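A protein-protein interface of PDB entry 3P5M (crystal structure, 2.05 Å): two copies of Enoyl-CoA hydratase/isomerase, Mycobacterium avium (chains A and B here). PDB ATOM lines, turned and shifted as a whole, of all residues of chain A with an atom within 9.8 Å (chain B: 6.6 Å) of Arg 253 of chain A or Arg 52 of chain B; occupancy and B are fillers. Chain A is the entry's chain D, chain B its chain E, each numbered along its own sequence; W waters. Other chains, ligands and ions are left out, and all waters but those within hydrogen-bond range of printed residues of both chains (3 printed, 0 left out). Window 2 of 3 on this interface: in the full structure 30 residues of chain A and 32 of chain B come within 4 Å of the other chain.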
ATOM      1  N   THR A 130      22.073  12.232 -29.178  1.00  0.00           N
ATOM      2  CA  THR A 130      21.515  10.908 -28.856  1.00  0.00           C
ATOM      3  C   THR A 130      22.106  10.315 -27.586  1.00  0.00           C
ATOM      4  O   THR A 130      21.540   9.397 -27.007  1.00  0.00           O
ATOM      5  CB  THR A 130      21.655   9.880 -30.047  1.00  0.00           C
ATOM      6  OG1 THR A 130      23.031   9.795 -30.421  1.00  0.00           O
ATOM      7  CG2 THR A 130      20.788  10.306 -31.232  1.00  0.00           C
ATOM      8  N   GLY A 133      19.447  11.112 -25.454  1.00  0.00           N
ATOM      9  CA  GLY A 133      18.145  10.704 -25.948  1.00  0.00           C
ATOM     10  C   GLY A 133      17.417  11.703 -26.835  1.00  0.00           C
ATOM     11  O   GLY A 133      16.195  11.607 -27.018  1.00  0.00           O
ATOM     12  N   MET A 158      23.661   8.832 -35.200  1.00  0.00           N
ATOM     13  CA  MET A 158      23.296   7.632 -34.502  1.00  0.00           C
ATOM     14  C   MET A 158      24.343   7.113 -33.509  1.00  0.00           C
ATOM     15  O   MET A 158      23.967   6.516 -32.524  1.00  0.00           O
ATOM     16  CB  MET A 158      22.855   6.545 -35.464  1.00  0.00           C
ATOM     17  CG  MET A 158      21.447   6.795 -36.007  1.00  0.00           C
ATOM     18  SD  MET A 158      21.067   5.483 -37.136  1.00  0.00           S
ATOM     19  CE  MET A 158      19.440   6.026 -37.701  1.00  0.00           C
ATOM     20  N   THR A 234      10.139  11.630 -23.258  1.00  0.00           N
ATOM     21  CA  THR A 234      10.435  10.203 -23.188  1.00  0.00           C
ATOM     22  C   THR A 234      11.169   9.816 -21.901  1.00  0.00           C
ATOM     23  O   THR A 234      11.870  10.641 -21.287  1.00  0.00           O
ATOM     24  CB  THR A 234      11.249   9.710 -24.426  1.00  0.00           C
ATOM     25  OG1 THR A 234      12.520  10.394 -24.482  1.00  0.00           O
ATOM     26  CG2 THR A 234      10.443   9.983 -25.703  1.00  0.00           C
ATOM     27  N   ALA A 235      11.041   8.547 -21.523  1.00  0.00           N
ATOM     28  CA  ALA A 235      11.847   8.031 -20.418  1.00  0.00           C
ATOM     29  C   ALA A 235      13.328   8.096 -20.809  1.00  0.00           C
ATOM     30  O   ALA A 235      14.220   8.381 -19.969  1.00  0.00           O
ATOM     31  CB  ALA A 235      11.389   6.596 -20.007  1.00  0.00           C
ATOM     32  N   ASP A 236      13.610   7.884 -22.092  1.00  0.00           N
ATOM     33  CA  ASP A 236      15.002   7.903 -22.550  1.00  0.00           C
ATOM     34  C   ASP A 236      15.674   9.279 -22.368  1.00  0.00           C
ATOM     35  O   ASP A 236      16.851   9.338 -22.000  1.00  0.00           O
ATOM     36  CB  ASP A 236      15.112   7.453 -24.017  1.00  0.00           C
ATOM     37  CG  ASP A 236      15.065   5.911 -24.180  1.00  0.00           C
ATOM     38  OD1 ASP A 236      15.075   5.138 -23.198  1.00  0.00           O
ATOM     39  OD2 ASP A 236      14.992   5.461 -25.329  1.00  0.00           O
ATOM     40  N   PHE A 237      14.963  10.378 -22.642  1.00  0.00           N
ATOM     41  CA  PHE A 237      15.498  11.698 -22.296  1.00  0.00           C
ATOM     42  C   PHE A 237      15.663  11.845 -20.775  1.00  0.00           C
ATOM     43  O   PHE A 237      16.693  12.310 -20.296  1.00  0.00           O
ATOM     44  CB  PHE A 237      14.622  12.860 -22.823  1.00  0.00           C
ATOM     45  CG  PHE A 237      15.112  14.221 -22.375  1.00  0.00           C
ATOM     46  CD1 PHE A 237      16.377  14.686 -22.746  1.00  0.00           C
ATOM     47  CD2 PHE A 237      14.326  15.023 -21.559  1.00  0.00           C
ATOM     48  CE1 PHE A 237      16.824  15.919 -22.340  1.00  0.00           C
ATOM     49  CE2 PHE A 237      14.774  16.275 -21.142  1.00  0.00           C
ATOM     50  CZ  PHE A 237      16.031  16.722 -21.533  1.00  0.00           C
ATOM     51  N   ARG A 238      14.633  11.470 -20.017  1.00  0.00           N
ATOM     52  CA  ARG A 238      14.734  11.533 -18.570  1.00  0.00           C
ATOM     53  C   ARG A 238      16.020  10.856 -18.055  1.00  0.00           C
ATOM     54  O   ARG A 238      16.801  11.460 -17.323  1.00  0.00           O
ATOM     55  CB  ARG A 238      13.492  10.907 -17.929  1.00  0.00           C
ATOM     56  CG  ARG A 238      13.377  11.192 -16.468  1.00  0.00           C
ATOM     57  CD  ARG A 238      12.377  10.241 -15.821  1.00  0.00           C
ATOM     58  NE  ARG A 238      12.909   8.900 -15.643  1.00  0.00           N
ATOM     59  CZ  ARG A 238      12.281   7.775 -15.986  1.00  0.00           C
ATOM     60  NH1 ARG A 238      11.078   7.813 -16.562  1.00  0.00           N
ATOM     61  NH2 ARG A 238      12.867   6.603 -15.738  1.00  0.00           N
ATOM     62  N   GLU A 239      16.232   9.603 -18.446  1.00  0.00           N
ATOM     63  CA  GLU A 239      17.452   8.882 -18.102  1.00  0.00           C
ATOM     64  C   GLU A 239      18.727   9.513 -18.690  1.00  0.00           C
ATOM     65  O   GLU A 239      19.736   9.585 -18.024  1.00  0.00           O
ATOM     66  CB  GLU A 239      17.335   7.432 -18.536  1.00  0.00           C
ATOM     67  CG  GLU A 239      16.310   6.651 -17.733  1.00  0.00           C
ATOM     68  CD  GLU A 239      16.630   6.671 -16.231  1.00  0.00           C
ATOM     69  OE1 GLU A 239      17.822   6.473 -15.896  1.00  0.00           O
ATOM     70  OE2 GLU A 239      15.698   6.897 -15.406  1.00  0.00           O
ATOM     71  N   GLY A 240      18.665   9.931 -19.950  1.00  0.00           N
ATOM     72  CA  GLY A 240      19.826  10.542 -20.621  1.00  0.00           C
ATOM     73  C   GLY A 240      20.332  11.804 -19.935  1.00  0.00           C
ATOM     74  O   GLY A 240      21.538  11.937 -19.679  1.00  0.00           O
ATOM     75  N   PRO A 250      23.940   6.196 -19.772  1.00  0.00           N
ATOM     76  CA  PRO A 250      22.494   6.099 -19.727  1.00  0.00           C
ATOM     77  C   PRO A 250      21.985   4.719 -20.109  1.00  0.00           C
ATOM     78  O   PRO A 250      22.548   4.042 -20.976  1.00  0.00           O
ATOM     79  CB  PRO A 250      22.022   7.133 -20.765  1.00  0.00           C
ATOM     80  CG  PRO A 250      23.175   7.237 -21.760  1.00  0.00           C
ATOM     81  CD  PRO A 250      24.409   7.066 -20.881  1.00  0.00           C
ATOM     82  N   ASN A 251      20.899   4.343 -19.442  1.00  0.00           N
ATOM     83  CA  ASN A 251      20.107   3.208 -19.768  1.00  0.00           C
ATOM     84  C   ASN A 251      18.965   3.597 -20.700  1.00  0.00           C
ATOM     85  O   ASN A 251      17.918   4.046 -20.230  1.00  0.00           O
ATOM     86  CB  ASN A 251      19.501   2.667 -18.477  1.00  0.00           C
ATOM     87  CG  ASN A 251      18.876   1.298 -18.669  1.00  0.00           C
ATOM     88  OD1 ASN A 251      18.285   1.011 -19.706  1.00  0.00           O
ATOM     89  ND2 ASN A 251      19.016   0.446 -17.669  1.00  0.00           N
ATOM     90  N   PHE A 252      19.149   3.391 -22.002  1.00  0.00           N
ATOM     91  CA  PHE A 252      18.079   3.639 -22.983  1.00  0.00           C
ATOM     92  C   PHE A 252      17.185   2.439 -23.270  1.00  0.00           C
ATOM     93  O   PHE A 252      17.658   1.312 -23.426  1.00  0.00           O
ATOM     94  CB  PHE A 252      18.656   4.170 -24.300  1.00  0.00           C
ATOM     95  CG  PHE A 252      19.286   5.532 -24.173  1.00  0.00           C
ATOM     96  CD1 PHE A 252      18.607   6.568 -23.538  1.00  0.00           C
ATOM     97  CD2 PHE A 252      20.573   5.768 -24.666  1.00  0.00           C
ATOM     98  CE1 PHE A 252      19.206   7.851 -23.430  1.00  0.00           C
ATOM     99  CE2 PHE A 252      21.165   7.017 -24.575  1.00  0.00           C
ATOM    100  CZ  PHE A 252      20.476   8.071 -23.943  1.00  0.00           C
ATOM    101  N   ARG A 253      15.882   2.685 -23.379  1.00  0.00           N
ATOM    102  CA  ARG A 253      14.975   1.582 -23.626  1.00  0.00           C
ATOM    103  C   ARG A 253      14.120   1.715 -24.864  1.00  0.00           C
ATOM    104  O   ARG A 253      13.362   0.806 -25.145  1.00  0.00           O
ATOM    105  CB  ARG A 253      14.089   1.345 -22.396  1.00  0.00           C
ATOM    106  CG  ARG A 253      14.922   0.665 -21.283  1.00  0.00           C
ATOM    107  CD  ARG A 253      14.252   0.745 -20.000  1.00  0.00           C
ATOM    108  NE  ARG A 253      14.250   2.122 -19.487  1.00  0.00           N
ATOM    109  CZ  ARG A 253      13.502   2.511 -18.460  1.00  0.00           C
ATOM    110  NH1 ARG A 253      12.715   1.625 -17.859  1.00  0.00           N
ATOM    111  NH2 ARG A 253      13.535   3.774 -18.037  1.00  0.00           N
ATOM    112  N   GLY A 254      14.246   2.840 -25.571  1.00  0.00           N
ATOM    113  CA  GLY A 254      13.429   3.148 -26.740  1.00  0.00           C
ATOM    114  C   GLY A 254      12.012   3.608 -26.411  1.00  0.00           C
ATOM    115  O   GLY A 254      11.080   3.324 -27.168  1.00  0.00           O
ATOM    116  N   HIS A 255      11.828   4.250 -25.263  1.00  0.00           N
ATOM    117  CA  HIS A 255      10.564   4.932 -24.952  1.00  0.00           C
ATOM    118  C   HIS A 255      10.815   6.123 -23.995  1.00  0.00           C
ATOM    119  O   HIS A 255       9.903   6.839 -23.548  1.00  0.00           O
ATOM    120  CB  HIS A 255       9.485   3.947 -24.450  1.00  0.00           C
ATOM    121  CG  HIS A 255       9.762   3.362 -23.101  1.00  0.00           C
ATOM    122  ND1 HIS A 255      10.119   2.041 -22.922  1.00  0.00           N
ATOM    123  CD2 HIS A 255       9.718   3.910 -21.860  1.00  0.00           C
ATOM    124  CE1 HIS A 255      10.284   1.799 -21.631  1.00  0.00           C
ATOM    125  NE2 HIS A 255      10.055   2.919 -20.964  1.00  0.00           N
ATOM    126  OXT HIS A 255      12.003   6.391 -23.690  1.00  0.00           O
ATOM    127  N   GLY B  14      17.285 -10.863 -29.002  1.00  0.00           N
ATOM    128  CA  GLY B  14      17.169  -9.757 -28.044  1.00  0.00           C
ATOM    129  C   GLY B  14      16.343  -8.667 -28.681  1.00  0.00           C
ATOM    130  O   GLY B  14      15.205  -8.908 -29.091  1.00  0.00           O
ATOM    131  N   ALA B  15      16.928  -7.477 -28.829  1.00  0.00           N
ATOM    132  CA  ALA B  15      16.195  -6.338 -29.370  1.00  0.00           C
ATOM    133  C   ALA B  15      16.408  -6.169 -30.873  1.00  0.00           C
ATOM    134  O   ALA B  15      15.961  -5.160 -31.475  1.00  0.00           O
ATOM    135  CB  ALA B  15      16.600  -5.058 -28.629  1.00  0.00           C
ATOM    136  N   VAL B  16      17.126  -7.129 -31.460  1.00  0.00           N
ATOM    137  CA  VAL B  16      17.481  -7.076 -32.876  1.00  0.00           C
ATOM    138  C   VAL B  16      16.556  -8.005 -33.629  1.00  0.00           C
ATOM    139  O   VAL B  16      16.426  -9.176 -33.258  1.00  0.00           O
ATOM    140  CB  VAL B  16      18.965  -7.520 -33.151  1.00  0.00           C
ATOM    141  CG1 VAL B  16      19.268  -7.541 -34.651  1.00  0.00           C
ATOM    142  CG2 VAL B  16      19.986  -6.614 -32.415  1.00  0.00           C
ATOM    143  N   LEU B  17      15.927  -7.498 -34.693  1.00  0.00           N
ATOM    144  CA  LEU B  17      15.286  -8.382 -35.651  1.00  0.00           C
ATOM    145  C   LEU B  17      16.296  -8.722 -36.767  1.00  0.00           C
ATOM    146  O   LEU B  17      16.668  -7.860 -37.561  1.00  0.00           O
ATOM    147  CB  LEU B  17      13.985  -7.781 -36.232  1.00  0.00           C
ATOM    148  CG  LEU B  17      13.254  -8.709 -37.208  1.00  0.00           C
ATOM    149  CD1 LEU B  17      12.588  -9.920 -36.478  1.00  0.00           C
ATOM    150  CD2 LEU B  17      12.231  -7.942 -37.980  1.00  0.00           C
ATOM    151  N   ALA B  45       8.375  -4.849 -38.533  1.00  0.00           N
ATOM    152  CA  ALA B  45       9.294  -4.439 -37.458  1.00  0.00           C
ATOM    153  C   ALA B  45       8.764  -3.199 -36.748  1.00  0.00           C
ATOM    154  O   ALA B  45       9.018  -3.011 -35.565  1.00  0.00           O
ATOM    155  CB  ALA B  45      10.695  -4.185 -37.999  1.00  0.00           C
ATOM    156  N   ASP B  48       6.355  -4.124 -33.923  1.00  0.00           N
ATOM    157  CA  ASP B  48       6.892  -5.117 -33.013  1.00  0.00           C
ATOM    158  C   ASP B  48       7.676  -4.390 -31.916  1.00  0.00           C
ATOM    159  O   ASP B  48       8.798  -3.915 -32.159  1.00  0.00           O
ATOM    160  CB  ASP B  48       7.749  -6.100 -33.823  1.00  0.00           C
ATOM    161  CG  ASP B  48       8.267  -7.264 -33.004  1.00  0.00           C
ATOM    162  OD1 ASP B  48       8.302  -7.202 -31.734  1.00  0.00           O
ATOM    163  OD2 ASP B  48       8.689  -8.231 -33.674  1.00  0.00           O
ATOM    164  N   GLU B  49       7.077  -4.294 -30.718  1.00  0.00           N
ATOM    165  CA  GLU B  49       7.685  -3.563 -29.592  1.00  0.00           C
ATOM    166  C   GLU B  49       8.949  -4.184 -29.024  1.00  0.00           C
ATOM    167  O   GLU B  49       9.733  -3.495 -28.366  1.00  0.00           O
ATOM    168  CB  GLU B  49       6.674  -3.266 -28.471  1.00  0.00           C
ATOM    169  CG  GLU B  49       5.748  -2.123 -28.834  1.00  0.00           C
ATOM    170  CD  GLU B  49       4.822  -1.708 -27.708  1.00  0.00           C
ATOM    171  OE1 GLU B  49       5.283  -0.957 -26.819  1.00  0.00           O
ATOM    172  OE2 GLU B  49       3.634  -2.113 -27.739  1.00  0.00           O
ATOM    173  N   SER B  50       9.196  -5.459 -29.294  1.00  0.00           N
ATOM    174  CA  SER B  50      10.466  -6.019 -28.865  1.00  0.00           C
ATOM    175  C   SER B  50      11.651  -5.589 -29.790  1.00  0.00           C
ATOM    176  O   SER B  50      12.816  -5.671 -29.396  1.00  0.00           O
ATOM    177  CB  SER B  50      10.370  -7.540 -28.727  1.00  0.00           C
ATOM    178  OG  SER B  50      10.396  -8.136 -30.002  1.00  0.00           O
ATOM    179  N   VAL B  51      11.348  -5.115 -31.003  1.00  0.00           N
ATOM    180  CA  VAL B  51      12.395  -4.826 -31.972  1.00  0.00           C
ATOM    181  C   VAL B  51      12.925  -3.382 -31.835  1.00  0.00           C
ATOM    182  O   VAL B  51      12.170  -2.436 -31.947  1.00  0.00           O
ATOM    183  CB  VAL B  51      11.896  -5.070 -33.410  1.00  0.00           C
ATOM    184  CG1 VAL B  51      12.894  -4.544 -34.439  1.00  0.00           C
ATOM    185  CG2 VAL B  51      11.638  -6.575 -33.632  1.00  0.00           C
ATOM    186  N   ARG B  52      14.231  -3.230 -31.638  1.00  0.00           N
ATOM    187  CA  ARG B  52      14.824  -1.893 -31.629  1.00  0.00           C
ATOM    188  C   ARG B  52      15.815  -1.582 -32.746  1.00  0.00           C
ATOM    189  O   ARG B  52      16.221  -0.428 -32.908  1.00  0.00           O
ATOM    190  CB  ARG B  52      15.421  -1.585 -30.261  1.00  0.00           C
ATOM    191  CG  ARG B  52      14.344  -1.150 -29.307  1.00  0.00           C
ATOM    192  CD  ARG B  52      14.775  -1.211 -27.880  1.00  0.00           C
ATOM    193  NE  ARG B  52      15.735  -0.174 -27.533  1.00  0.00           N
ATOM    194  CZ  ARG B  52      16.501  -0.242 -26.452  1.00  0.00           C
ATOM    195  NH1 ARG B  52      16.360  -1.277 -25.620  1.00  0.00           N
ATOM    196  NH2 ARG B  52      17.376   0.729 -26.182  1.00  0.00           N
ATOM    197  N   ALA B  53      16.239  -2.616 -33.475  1.00  0.00           N
ATOM    198  CA  ALA B  53      17.090  -2.446 -34.664  1.00  0.00           C
ATOM    199  C   ALA B  53      16.786  -3.585 -35.583  1.00  0.00           C
ATOM    200  O   ALA B  53      16.396  -4.660 -35.144  1.00  0.00           O
ATOM    201  CB  ALA B  53      18.601  -2.449 -34.297  1.00  0.00           C
ATOM    202  N   VAL B  54      16.945  -3.362 -36.868  1.00  0.00           N
ATOM    203  CA  VAL B  54      16.833  -4.464 -37.830  1.00  0.00           C
ATOM    204  C   VAL B  54      18.218  -4.734 -38.406  1.00  0.00           C
ATOM    205  O   VAL B  54      18.956  -3.788 -38.778  1.00  0.00           O
ATOM    206  CB  VAL B  54      15.854  -4.124 -38.906  1.00  0.00           C
ATOM    207  CG1 VAL B  54      15.844  -5.204 -39.986  1.00  0.00           C
ATOM    208  CG2 VAL B  54      14.467  -3.961 -38.303  1.00  0.00           C
ATOM    209  N   LYS B  93      12.936   2.916 -37.048  1.00  0.00           N
ATOM    210  CA  LYS B  93      13.943   2.152 -36.285  1.00  0.00           C
ATOM    211  C   LYS B  93      15.189   1.997 -37.139  1.00  0.00           C
ATOM    212  O   LYS B  93      15.050   1.808 -38.333  1.00  0.00           O
ATOM    213  CB  LYS B  93      13.399   0.757 -35.957  1.00  0.00           C
ATOM    214  CG  LYS B  93      12.160   0.845 -35.025  1.00  0.00           C
ATOM    215  CD  LYS B  93      11.587  -0.493 -34.606  1.00  0.00           C
ATOM    216  CE  LYS B  93      10.349  -0.298 -33.660  1.00  0.00           C
ATOM    217  NZ  LYS B  93       9.646  -1.614 -33.386  1.00  0.00           N
ATOM    218  N   PRO B  94      16.404   2.035 -36.536  1.00  0.00           N
ATOM    219  CA  PRO B  94      17.664   1.794 -37.306  1.00  0.00           C
ATOM    220  C   PRO B  94      17.709   0.436 -38.009  1.00  0.00           C
ATOM    221  O   PRO B  94      17.374  -0.573 -37.404  1.00  0.00           O
ATOM    222  CB  PRO B  94      18.759   1.814 -36.236  1.00  0.00           C
ATOM    223  CG  PRO B  94      18.003   1.592 -34.901  1.00  0.00           C
ATOM    224  CD  PRO B  94      16.649   2.203 -35.099  1.00  0.00           C
ATOM    225  N   VAL B 194      23.614  -0.075 -31.056  1.00  0.00           N
ATOM    226  CA  VAL B 194      22.489   0.620 -31.698  1.00  0.00           C
ATOM    227  C   VAL B 194      21.138   0.088 -31.164  1.00  0.00           C
ATOM    228  O   VAL B 194      20.245   0.871 -30.868  1.00  0.00           O
ATOM    229  CB  VAL B 194      22.529   0.516 -33.255  1.00  0.00           C
ATOM    230  CG1 VAL B 194      21.220   1.033 -33.850  1.00  0.00           C
ATOM    231  CG2 VAL B 194      23.726   1.314 -33.836  1.00  0.00           C
ATOM    232  N   SER B 195      21.006  -1.230 -31.024  1.00  0.00           N
ATOM    233  CA  SER B 195      19.788  -1.835 -30.441  1.00  0.00           C
ATOM    234  C   SER B 195      19.562  -1.519 -28.937  1.00  0.00           C
ATOM    235  O   SER B 195      18.496  -1.751 -28.405  1.00  0.00           O
ATOM    236  CB  SER B 195      19.780  -3.360 -30.712  1.00  0.00           C
ATOM    237  OG  SER B 195      20.760  -4.044 -29.934  1.00  0.00           O
ATOM    238  N   GLY B 196      20.565  -0.987 -28.255  1.00  0.00           N
ATOM    239  CA  GLY B 196      20.420  -0.541 -26.869  1.00  0.00           C
ATOM    240  C   GLY B 196      20.338   0.980 -26.753  1.00  0.00           C
ATOM    241  O   GLY B 196      20.334   1.507 -25.645  1.00  0.00           O
ATOM    242  N   GLY B 197      20.288   1.667 -27.899  1.00  0.00           N
ATOM    243  CA  GLY B 197      20.293   3.146 -27.967  1.00  0.00           C
ATOM    244  C   GLY B 197      18.890   3.764 -27.850  1.00  0.00           C
ATOM    245  O   GLY B 197      17.918   3.041 -27.718  1.00  0.00           O
ATOM    246  N   PRO B 198      18.791   5.110 -27.895  1.00  0.00           N
ATOM    247  CA  PRO B 198      17.492   5.772 -27.769  1.00  0.00           C
ATOM    248  C   PRO B 198      16.716   5.613 -29.083  1.00  0.00           C
ATOM    249  O   PRO B 198      16.787   6.456 -29.963  1.00  0.00           O
ATOM    250  CB  PRO B 198      17.874   7.236 -27.485  1.00  0.00           C
ATOM    251  CG  PRO B 198      19.172   7.429 -28.216  1.00  0.00           C
ATOM    252  CD  PRO B 198      19.870   6.071 -28.204  1.00  0.00           C
ATOM    253  N   THR B 199      15.994   4.505 -29.201  1.00  0.00           N
ATOM    254  CA  THR B 199      15.313   4.136 -30.437  1.00  0.00           C
ATOM    255  C   THR B 199      14.340   5.221 -30.970  1.00  0.00           C
ATOM    256  O   THR B 199      14.269   5.463 -32.191  1.00  0.00           O
ATOM    257  CB  THR B 199      14.565   2.781 -30.207  1.00  0.00           C
ATOM    258  OG1 THR B 199      15.469   1.838 -29.608  1.00  0.00           O
ATOM    259  CG2 THR B 199      14.035   2.213 -31.525  1.00  0.00           C
ATOM    260  N   PHE B 202      16.336   7.902 -32.586  1.00  0.00           N
ATOM    261  CA  PHE B 202      16.783   7.388 -33.883  1.00  0.00           C
ATOM    262  C   PHE B 202      15.664   7.472 -34.926  1.00  0.00           C
ATOM    263  O   PHE B 202      15.905   7.885 -36.049  1.00  0.00           O
ATOM    264  CB  PHE B 202      17.225   5.934 -33.776  1.00  0.00           C
ATOM    265  CG  PHE B 202      18.501   5.726 -33.003  1.00  0.00           C
ATOM    266  CD1 PHE B 202      19.437   6.769 -32.832  1.00  0.00           C
ATOM    267  CD2 PHE B 202      18.770   4.480 -32.451  1.00  0.00           C
ATOM    268  CE1 PHE B 202      20.596   6.565 -32.105  1.00  0.00           C
ATOM    269  CE2 PHE B 202      19.949   4.249 -31.715  1.00  0.00           C
ATOM    270  CZ  PHE B 202      20.875   5.287 -31.542  1.00  0.00           C
HETATM  271  O   HOH W   1      14.496   6.926 -27.456  1.00  0.00           O
HETATM  272  O   HOH W   2      18.402  -1.867 -23.855  1.00  0.00           O
HETATM  273  O   HOH W   3      20.838   1.369 -23.146  1.00  0.00           O
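NH2 of Arg 52 of chain B is in hydrogen-bond range of O of Phe 252 of chain A (2.8 Å).
O of Gly 196 of chain B lies close to O of Phe 252 of chain A.
N of Arg 253 of chain A lies within hydrogen-bond range of OD1 of Asp 236 of chain A, at 2.6 Å.
OD2 of Asp 236 of chain A is in hydrogen-bond range of N of Gly 254 of chain A (2.7 Å).
O of Ala 15 of chain B is in hydrogen-bond range of N of Arg 52 of chain B, 2.6 Å away.
NE of Arg 52 of chain B lies close to O of Ser 195 of chain B.
O of Gly 197 of chain B is in hydrogen-bond range of NH2 of Arg 52 of chain B, 2.8 Å away.
The side-chain hydroxyl (OG1) of Thr 199 of chain B is in hydrogen-bond range of the backbone carbonyl oxygen (O) of Gly 197 of chain B, 3.3 Å away.
CG of Pro 198 of chain B touches O of Thr 130 of chain A, at 3.3 Å.
Thr 130 of chain A touches Phe 202 of chain B (CG2 to CE1, 3.8 Å).
Pro 198 of chain B touches Gly 133 of chain A.
Met 158 of chain A touches Phe 202 of chain B (O to CE1, 3.4 Å).
OD2 of Asp 236 of chain A touches CA of Pro 198 of chain B, 3.5 Å away.
Phe 252 of chain A touches Gly 197 of chain B.
CD2 of Phe 252 of chain A touches CD of Pro 198 of chain B (3.6 Å).
Arg 52 of chain B touches Arg 253 of chain A (CZ to C, 3.5 Å).
Arg 52 of chain B touches Gly 254 of chain A (NH2 to N, 3.8 Å).
Gly 254 of chain A touches Thr 199 of chain B (CA to CB, 3.7 Å).
Of the printed residues of chain B, Met 158 of chain A touches Phe 202 (3.4 Å).
Arg 238 of chain A touches none of the printed residues of chain B.
Of chain B, only Arg 52 comes within 4 Å of Arg 253 of chain A.
No residue of chain A comes within 4 Å of Val 51 of chain B.
Of chain A, only Phe 252, Arg 253 and Gly 254 come within 4 Å of Arg 52 of chain B.
No residue of chain A comes within 4 Å of Pro 94 of chain B.
Of chain A, only Phe 252 comes within 4 Å of Gly 196 of chain B.
Of the printed residues of chain A, Phe 202 of chain B touches Thr 130 (3.8 Å) and Met 158 (3.4 Å).
The nearest residue of chain A that does not touch Arg 52 of chain B is Asp 236 of chain A (5.4 Å).
Of the 21 printed residues of chain B, 6 touch a printed residue of chain A.
Among the printed residues, 12 pairs touch across the chains.
Among the printed residues, no Asp or Glu carboxylate lies within 4 Å of a Lys or Arg side-chain nitrogen of the other chain.
No position is printed for both chains.
Of the 12 pairs that touch across the chains among the printed residues, none has its exchanged pair printed and touching as well.
Water W3 bridges the backbone carbonyl oxygen (O) of Gly 196 of chain B (2.6 Å) and the backbone NH (N) of Phe 252 of chain A (2.9 Å).
Water W1 lies within hydrogen-bond range of OD2 of Asp 236 of chain A (2.6 Å), N of Thr 199 of chain B (3.3 Å) and O of Pro 198 of chain B (3.4 Å).
Water W2 bridges NH1 of Arg 52 of chain B (2.8 Å) and O of Phe 252 of chain A (3.3 Å).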
